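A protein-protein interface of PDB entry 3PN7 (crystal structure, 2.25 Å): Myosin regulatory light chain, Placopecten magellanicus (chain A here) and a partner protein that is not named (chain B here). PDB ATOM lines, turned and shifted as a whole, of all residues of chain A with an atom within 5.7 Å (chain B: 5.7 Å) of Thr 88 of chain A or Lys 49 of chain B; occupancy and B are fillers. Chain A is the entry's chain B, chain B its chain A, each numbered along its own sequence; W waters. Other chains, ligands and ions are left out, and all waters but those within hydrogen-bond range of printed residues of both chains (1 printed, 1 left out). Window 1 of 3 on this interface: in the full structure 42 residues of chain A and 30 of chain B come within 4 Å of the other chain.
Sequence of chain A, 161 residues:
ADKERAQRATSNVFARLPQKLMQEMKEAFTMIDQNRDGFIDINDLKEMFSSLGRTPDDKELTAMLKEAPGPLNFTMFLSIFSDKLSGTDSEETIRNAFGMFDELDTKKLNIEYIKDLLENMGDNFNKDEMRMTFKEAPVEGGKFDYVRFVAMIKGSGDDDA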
ATOM      1  N   ARG A  16      11.148  39.514  -0.034  1.00  0.00           N
ATOM      2  CA  ARG A  16      12.167  39.847  -1.020  1.00  0.00           C
ATOM      3  C   ARG A  16      11.531  40.337  -2.313  1.00  0.00           C
ATOM      4  O   ARG A  16      10.468  40.953  -2.294  1.00  0.00           O
ATOM      5  CB  ARG A  16      13.061  38.638  -1.298  1.00  0.00           C
ATOM      6  CG  ARG A  16      13.928  38.222  -0.119  1.00  0.00           C
ATOM      7  CD  ARG A  16      14.851  37.050  -0.410  1.00  0.00           C
ATOM      8  NE  ARG A  16      15.610  36.646   0.770  1.00  0.00           N
ATOM      9  CZ  ARG A  16      16.398  35.582   0.820  1.00  0.00           C
ATOM     10  NH1 ARG A  16      16.541  34.808  -0.248  1.00  0.00           N
ATOM     11  NH2 ARG A  16      17.051  35.288   1.937  1.00  0.00           N
ATOM     12  N   LEU A  21      20.004  39.582  -5.747  1.00  0.00           N
ATOM     13  CA  LEU A  21      19.401  38.551  -6.576  1.00  0.00           C
ATOM     14  C   LEU A  21      18.765  39.181  -7.820  1.00  0.00           C
ATOM     15  O   LEU A  21      18.870  38.643  -8.919  1.00  0.00           O
ATOM     16  CB  LEU A  21      18.383  37.731  -5.776  1.00  0.00           C
ATOM     17  CG  LEU A  21      17.711  36.587  -6.540  1.00  0.00           C
ATOM     18  CD1 LEU A  21      18.750  35.578  -6.994  1.00  0.00           C
ATOM     19  CD2 LEU A  21      16.639  35.915  -5.687  1.00  0.00           C
ATOM     20  N   ASP A  83       9.747  33.505  -8.807  1.00  0.00           N
ATOM     21  CA  ASP A  83       9.172  32.617  -7.804  1.00  0.00           C
ATOM     22  C   ASP A  83      10.112  31.445  -7.504  1.00  0.00           C
ATOM     23  O   ASP A  83      10.262  31.030  -6.351  1.00  0.00           O
ATOM     24  CB  ASP A  83       7.784  32.117  -8.238  1.00  0.00           C
ATOM     25  CG  ASP A  83       6.760  33.244  -8.345  1.00  0.00           C
ATOM     26  OD1 ASP A  83       6.528  33.950  -7.342  1.00  0.00           O
ATOM     27  OD2 ASP A  83       6.201  33.449  -9.440  1.00  0.00           O
ATOM     28  N   LYS A  84      10.765  30.923  -8.533  1.00  0.00           N
ATOM     29  CA  LYS A  84      11.611  29.755  -8.323  1.00  0.00           C
ATOM     30  C   LYS A  84      12.941  30.107  -7.641  1.00  0.00           C
ATOM     31  O   LYS A  84      13.549  29.261  -7.013  1.00  0.00           O
ATOM     32  CB  LYS A  84      11.856  29.012  -9.632  1.00  0.00           C
ATOM     33  CG  LYS A  84      10.716  28.103 -10.066  1.00  0.00           C
ATOM     34  CD  LYS A  84      10.899  27.765 -11.542  1.00  0.00           C
ATOM     35  CE  LYS A  84       9.941  26.699 -12.008  1.00  0.00           C
ATOM     36  NZ  LYS A  84       8.543  27.209 -12.068  1.00  0.00           N
ATOM     37  N   LEU A  85      13.377  31.353  -7.761  1.00  0.00           N
ATOM     38  CA  LEU A  85      14.634  31.779  -7.147  1.00  0.00           C
ATOM     39  C   LEU A  85      14.449  32.551  -5.852  1.00  0.00           C
ATOM     40  O   LEU A  85      15.411  32.728  -5.114  1.00  0.00           O
ATOM     41  CB  LEU A  85      15.460  32.649  -8.100  1.00  0.00           C
ATOM     42  CG  LEU A  85      16.061  32.034  -9.368  1.00  0.00           C
ATOM     43  CD1 LEU A  85      16.920  33.053 -10.085  1.00  0.00           C
ATOM     44  CD2 LEU A  85      16.873  30.802  -9.050  1.00  0.00           C
ATOM     45  N   SER A  86      13.225  33.003  -5.576  1.00  0.00           N
ATOM     46  CA  SER A  86      13.013  33.998  -4.528  1.00  0.00           C
ATOM     47  C   SER A  86      13.673  33.653  -3.187  1.00  0.00           C
ATOM     48  O   SER A  86      14.413  34.474  -2.629  1.00  0.00           O
ATOM     49  CB  SER A  86      11.525  34.339  -4.350  1.00  0.00           C
ATOM     50  OG  SER A  86      10.787  33.230  -3.877  1.00  0.00           O
ATOM     51  N   GLY A  87      13.438  32.453  -2.667  1.00  0.00           N
ATOM     52  CA  GLY A  87      14.035  32.118  -1.381  1.00  0.00           C
ATOM     53  C   GLY A  87      15.421  31.483  -1.424  1.00  0.00           C
ATOM     54  O   GLY A  87      15.848  30.875  -0.443  1.00  0.00           O
ATOM     55  N   THR A  88      16.132  31.593  -2.542  1.00  0.00           N
ATOM     56  CA  THR A  88      17.445  30.945  -2.623  1.00  0.00           C
ATOM     57  C   THR A  88      18.564  31.820  -2.082  1.00  0.00           C
ATOM     58  O   THR A  88      18.499  33.048  -2.134  1.00  0.00           O
ATOM     59  CB  THR A  88      17.805  30.475  -4.034  1.00  0.00           C
ATOM     60  OG1 THR A  88      17.895  31.602  -4.922  1.00  0.00           O
ATOM     61  CG2 THR A  88      16.772  29.471  -4.542  1.00  0.00           C
ATOM     62  N   ASP A  89      19.596  31.172  -1.562  1.00  0.00           N
ATOM     63  CA  ASP A  89      20.676  31.887  -0.913  1.00  0.00           C
ATOM     64  C   ASP A  89      21.979  31.523  -1.576  1.00  0.00           C
ATOM     65  O   ASP A  89      22.056  30.536  -2.305  1.00  0.00           O
ATOM     66  CB  ASP A  89      20.722  31.551   0.583  1.00  0.00           C
ATOM     67  CG  ASP A  89      19.475  31.992   1.313  1.00  0.00           C
ATOM     68  OD1 ASP A  89      19.341  33.215   1.535  1.00  0.00           O
ATOM     69  OD2 ASP A  89      18.624  31.130   1.657  1.00  0.00           O
ATOM     70  N   SER A  90      23.004  32.326  -1.322  1.00  0.00           N
ATOM     71  CA  SER A  90      24.319  32.065  -1.904  1.00  0.00           C
ATOM     72  C   SER A  90      24.916  30.766  -1.357  1.00  0.00           C
ATOM     73  O   SER A  90      24.559  30.302  -0.258  1.00  0.00           O
ATOM     74  CB  SER A  90      25.276  33.238  -1.634  1.00  0.00           C
ATOM     75  OG  SER A  90      25.638  33.272  -0.275  1.00  0.00           O
ATOM     76  N   LYS A 154      23.710  23.912  -6.062  1.00  0.00           N
ATOM     77  CA  LYS A 154      23.854  25.179  -6.770  1.00  0.00           C
ATOM     78  C   LYS A 154      24.419  24.997  -8.175  1.00  0.00           C
ATOM     79  O   LYS A 154      24.526  25.957  -8.932  1.00  0.00           O
ATOM     80  CB  LYS A 154      24.743  26.135  -5.976  1.00  0.00           C
ATOM     81  CG  LYS A 154      24.107  26.670  -4.707  1.00  0.00           C
ATOM     82  CD  LYS A 154      22.992  27.646  -5.021  1.00  0.00           C
ATOM     83  CE  LYS A 154      23.268  29.002  -4.410  1.00  0.00           C
ATOM     84  NZ  LYS A 154      22.406  30.054  -5.002  1.00  0.00           N
ATOM     85  N   GLN B  44      16.578  23.860   4.594  1.00  0.00           N
ATOM     86  CA  GLN B  44      15.387  23.173   4.098  1.00  0.00           C
ATOM     87  C   GLN B  44      14.824  23.877   2.854  1.00  0.00           C
ATOM     88  O   GLN B  44      14.450  23.233   1.887  1.00  0.00           O
ATOM     89  CB  GLN B  44      14.323  23.033   5.196  1.00  0.00           C
ATOM     90  CG  GLN B  44      14.762  22.109   6.343  1.00  0.00           C
ATOM     91  CD  GLN B  44      13.804  22.101   7.527  1.00  0.00           C
ATOM     92  OE1 GLN B  44      13.308  23.142   7.965  1.00  0.00           O
ATOM     93  NE2 GLN B  44      13.539  20.913   8.044  1.00  0.00           N
ATOM     94  N   ARG B  45      14.812  25.203   2.879  1.00  0.00           N
ATOM     95  CA  ARG B  45      14.254  25.992   1.788  1.00  0.00           C
ATOM     96  C   ARG B  45      15.104  25.915   0.519  1.00  0.00           C
ATOM     97  O   ARG B  45      14.576  25.709  -0.574  1.00  0.00           O
ATOM     98  CB  ARG B  45      14.108  27.429   2.257  1.00  0.00           C
ATOM     99  CG  ARG B  45      14.054  28.475   1.182  1.00  0.00           C
ATOM    100  CD  ARG B  45      13.843  29.836   1.842  1.00  0.00           C
ATOM    101  NE  ARG B  45      15.099  30.508   2.159  1.00  0.00           N
ATOM    102  CZ  ARG B  45      15.403  31.019   3.347  1.00  0.00           C
ATOM    103  NH1 ARG B  45      14.553  30.917   4.366  1.00  0.00           N
ATOM    104  NH2 ARG B  45      16.561  31.640   3.513  1.00  0.00           N
ATOM    105  N   ASN B  46      16.421  26.051   0.672  1.00  0.00           N
ATOM    106  CA  ASN B  46      17.330  25.868  -0.451  1.00  0.00           C
ATOM    107  C   ASN B  46      17.335  24.450  -1.059  1.00  0.00           C
ATOM    108  O   ASN B  46      17.397  24.291  -2.284  1.00  0.00           O
ATOM    109  CB  ASN B  46      18.735  26.347  -0.097  1.00  0.00           C
ATOM    110  CG  ASN B  46      18.880  27.849  -0.239  1.00  0.00           C
ATOM    111  OD1 ASN B  46      19.129  28.361  -1.329  1.00  0.00           O
ATOM    112  ND2 ASN B  46      18.732  28.564   0.868  1.00  0.00           N
ATOM    113  N   ILE B  47      17.255  23.417  -0.229  1.00  0.00           N
ATOM    114  CA  ILE B  47      17.120  22.078  -0.783  1.00  0.00           C
ATOM    115  C   ILE B  47      15.813  21.964  -1.557  1.00  0.00           C
ATOM    116  O   ILE B  47      15.800  21.439  -2.681  1.00  0.00           O
ATOM    117  CB  ILE B  47      17.168  20.976   0.281  1.00  0.00           C
ATOM    118  CG1 ILE B  47      18.566  20.888   0.906  1.00  0.00           C
ATOM    119  CG2 ILE B  47      16.780  19.632  -0.331  1.00  0.00           C
ATOM    120  CD1 ILE B  47      18.616  20.048   2.181  1.00  0.00           C
ATOM    121  N   ARG B  48      14.719  22.454  -0.967  1.00  0.00           N
ATOM    122  CA  ARG B  48      13.426  22.376  -1.641  1.00  0.00           C
ATOM    123  C   ARG B  48      13.405  23.124  -2.990  1.00  0.00           C
ATOM    124  O   ARG B  48      12.907  22.602  -3.982  1.00  0.00           O
ATOM    125  CB  ARG B  48      12.294  22.864  -0.728  1.00  0.00           C
ATOM    126  CG  ARG B  48      11.759  21.784   0.215  1.00  0.00           C
ATOM    127  CD  ARG B  48      10.817  22.372   1.264  1.00  0.00           C
ATOM    128  NE  ARG B  48      10.128  21.317   1.997  1.00  0.00           N
ATOM    129  CZ  ARG B  48      10.010  21.262   3.323  1.00  0.00           C
ATOM    130  NH1 ARG B  48      10.531  22.225   4.092  1.00  0.00           N
ATOM    131  NH2 ARG B  48       9.361  20.241   3.879  1.00  0.00           N
ATOM    132  N   LYS B  49      13.935  24.347  -3.013  1.00  0.00           N
ATOM    133  CA  LYS B  49      14.047  25.122  -4.252  1.00  0.00           C
ATOM    134  C   LYS B  49      14.818  24.325  -5.295  1.00  0.00           C
ATOM    135  O   LYS B  49      14.413  24.243  -6.455  1.00  0.00           O
ATOM    136  CB  LYS B  49      14.750  26.459  -4.004  1.00  0.00           C
ATOM    137  CG  LYS B  49      13.911  27.472  -3.224  1.00  0.00           C
ATOM    138  CD  LYS B  49      12.647  27.823  -3.972  1.00  0.00           C
ATOM    139  CE  LYS B  49      11.908  28.970  -3.312  1.00  0.00           C
ATOM    140  NZ  LYS B  49      10.656  29.299  -4.063  1.00  0.00           N
ATOM    141  N   TRP B  50      15.926  23.727  -4.870  1.00  0.00           N
ATOM    142  CA  TRP B  50      16.723  22.893  -5.758  1.00  0.00           C
ATOM    143  C   TRP B  50      15.927  21.721  -6.358  1.00  0.00           C
ATOM    144  O   TRP B  50      15.995  21.482  -7.564  1.00  0.00           O
ATOM    145  CB  TRP B  50      17.956  22.401  -5.029  1.00  0.00           C
ATOM    146  CG  TRP B  50      18.684  21.301  -5.717  1.00  0.00           C
ATOM    147  CD1 TRP B  50      19.424  21.390  -6.868  1.00  0.00           C
ATOM    148  CD2 TRP B  50      18.785  19.944  -5.279  1.00  0.00           C
ATOM    149  NE1 TRP B  50      19.961  20.163  -7.179  1.00  0.00           N
ATOM    150  CE2 TRP B  50      19.587  19.259  -6.219  1.00  0.00           C
ATOM    151  CE3 TRP B  50      18.270  19.236  -4.185  1.00  0.00           C
ATOM    152  CZ2 TRP B  50      19.881  17.898  -6.098  1.00  0.00           C
ATOM    153  CZ3 TRP B  50      18.568  17.886  -4.066  1.00  0.00           C
ATOM    154  CH2 TRP B  50      19.362  17.232  -5.018  1.00  0.00           C
ATOM    155  N   LEU B  51      15.168  21.007  -5.525  1.00  0.00           N
ATOM    156  CA  LEU B  51      14.415  19.832  -5.975  1.00  0.00           C
ATOM    157  C   LEU B  51      13.425  20.174  -7.097  1.00  0.00           C
ATOM    158  O   LEU B  51      13.055  19.322  -7.895  1.00  0.00           O
ATOM    159  CB  LEU B  51      13.645  19.209  -4.804  1.00  0.00           C
ATOM    160  CG  LEU B  51      14.425  18.554  -3.661  1.00  0.00           C
ATOM    161  CD1 LEU B  51      13.465  18.033  -2.610  1.00  0.00           C
ATOM    162  CD2 LEU B  51      15.281  17.424  -4.195  1.00  0.00           C
ATOM    163  N   VAL B  52      12.980  21.424  -7.127  1.00  0.00           N
ATOM    164  CA  VAL B  52      12.054  21.877  -8.153  1.00  0.00           C
ATOM    165  C   VAL B  52      12.801  22.340  -9.402  1.00  0.00           C
ATOM    166  O   VAL B  52      12.392  22.059 -10.527  1.00  0.00           O
ATOM    167  CB  VAL B  52      11.147  23.030  -7.653  1.00  0.00           C
ATOM    168  CG1 VAL B  52      10.605  23.823  -8.837  1.00  0.00           C
ATOM    169  CG2 VAL B  52      10.000  22.484  -6.797  1.00  0.00           C
ATOM    170  N   LEU B  53      13.911  23.032  -9.220  1.00  0.00           N
ATOM    171  CA  LEU B  53      14.521  23.633 -10.373  1.00  0.00           C
ATOM    172  C   LEU B  53      15.601  22.771 -11.064  1.00  0.00           C
ATOM    173  O   LEU B  53      16.022  23.075 -12.181  1.00  0.00           O
ATOM    174  CB  LEU B  53      14.927  25.081 -10.064  1.00  0.00           C
ATOM    175  CG  LEU B  53      16.293  25.595  -9.629  1.00  0.00           C
ATOM    176  CD1 LEU B  53      16.109  26.717  -8.583  1.00  0.00           C
ATOM    177  CD2 LEU B  53      17.203  24.484  -9.118  1.00  0.00           C
ATOM    178  N   ARG B  54      15.997  21.667 -10.442  1.00  0.00           N
ATOM    179  CA  ARG B  54      17.129  20.906 -10.956  1.00  0.00           C
ATOM    180  C   ARG B  54      16.887  20.295 -12.338  1.00  0.00           C
ATOM    181  O   ARG B  54      17.821  20.093 -13.088  1.00  0.00           O
ATOM    182  CB  ARG B  54      17.573  19.829  -9.971  1.00  0.00           C
ATOM    183  CG  ARG B  54      16.582  18.700  -9.790  1.00  0.00           C
ATOM    184  CD  ARG B  54      17.072  17.693  -8.748  1.00  0.00           C
ATOM    185  NE  ARG B  54      16.020  16.730  -8.432  1.00  0.00           N
ATOM    186  CZ  ARG B  54      16.222  15.579  -7.798  1.00  0.00           C
ATOM    187  NH1 ARG B  54      17.443  15.240  -7.406  1.00  0.00           N
ATOM    188  NH2 ARG B  54      15.205  14.761  -7.561  1.00  0.00           N
HETATM  189  O   HOH W   1      12.571  26.681  -7.141  1.00  0.00           O
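O of Gly 87 of chain A lies within hydrogen-bond range of NE of Arg 45 of chain B. ND2 of Asn 46 of chain B sits at hydrogen-bond distance from OD2 of Asp 89 of chain A, 2.7 Å away. OD2 of Asp 89 of chain A is in salt-bridge range of NH2 of Arg 45 of chain B, 2.8 Å away. NZ of Lys 49 of chain B lies within hydrogen-bond range of O of Asp 83 of chain A.
The backbone carbonyl oxygen (O) of Asp 83 of chain A lies within hydrogen-bond range of the side-chain hydroxyl (OG) of Ser 86 of chain A, at 3.4 Å. The guanidinium group (NH1) of Arg 16 of chain A is in hydrogen-bond range of the backbone carbonyl oxygen (O) of Ser 86 of chain A, at 3.2 Å. NH2 of Arg 16 of chain A lies within salt-bridge range of OD1 of Asp 89 of chain A. The backbone carbonyl oxygen of Leu 85 of chain A is in hydrogen-bond range of the side-chain hydroxyl of Thr 88 of chain A. O of Asp 89 of chain A lies within hydrogen-bond range of NZ of Lys 154 of chain A (2.8 Å). The guanidinium group (NH1) of Arg 16 of chain A lies within hydrogen-bond range of the backbone carbonyl oxygen (O) of Thr 88 of chain A (3.2 Å).
Lys 84 of chain A touches Lys 49 of chain B. Leu 53 of chain B touches Lys 84 of chain A. Ser 86 of chain A touches Lys 49 of chain B. O of Gly 87 of chain A touches ND2 of Asn 46 of chain B, at 3.9 Å. N of Gly 87 of chain A touches CE of Lys 49 of chain B (3.9 Å). Asn 46 of chain B touches Thr 88 of chain A. CG2 of Thr 88 of chain A touches CB of Lys 49 of chain B, 3.7 Å away.
Arg 16 of chain A touches none of the printed residues of chain B. Of the printed residues of chain B, Asp 83 of chain A touches Lys 49 (2.9 Å). Printed residues of chain B within 4 Å of Ser 86 of chain A: Lys 49 (3.9 Å). Thr 88 of chain A touches just these residues of chain B: Asn 46 (3.3 Å) and Lys 49 (3.7 Å). Of the printed residues of chain B, Asp 89 of chain A touches Arg 45 (2.8 Å) and Asn 46 (2.7 Å). Lys 154 of chain A touches none of the printed residues of chain B. Lys 49 of chain B touches just these residues of chain A: Asp 83, Lys 84, Ser 86, Gly 87 and Thr 88. The nearest printed residue of chain B that does not touch Thr 88 of chain A is Arg 45 of chain B (4.9 Å). The nearest printed residue of chain B that does not touch Lys 84 of chain A is Val 52 of chain B (4.3 Å).
Of the 11 printed residues of chain A, 6 touch a printed residue of chain B. Printed residues of chain A that touch a printed residue of chain B: Asp 83, Lys 84, Ser 86, Gly 87, Thr 88 and Asp 89. Hydrophobic or aromatic side chains of chain B within 4 Å of the printed part of chain A: Leu 53. Among the printed residues, 11 pairs touch across the chains.
Water W1 bridges the backbone carbonyl oxygen (O) of Lys 84 of chain A and the backbone carbonyl oxygen (O) of Lys 49 of chain B.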
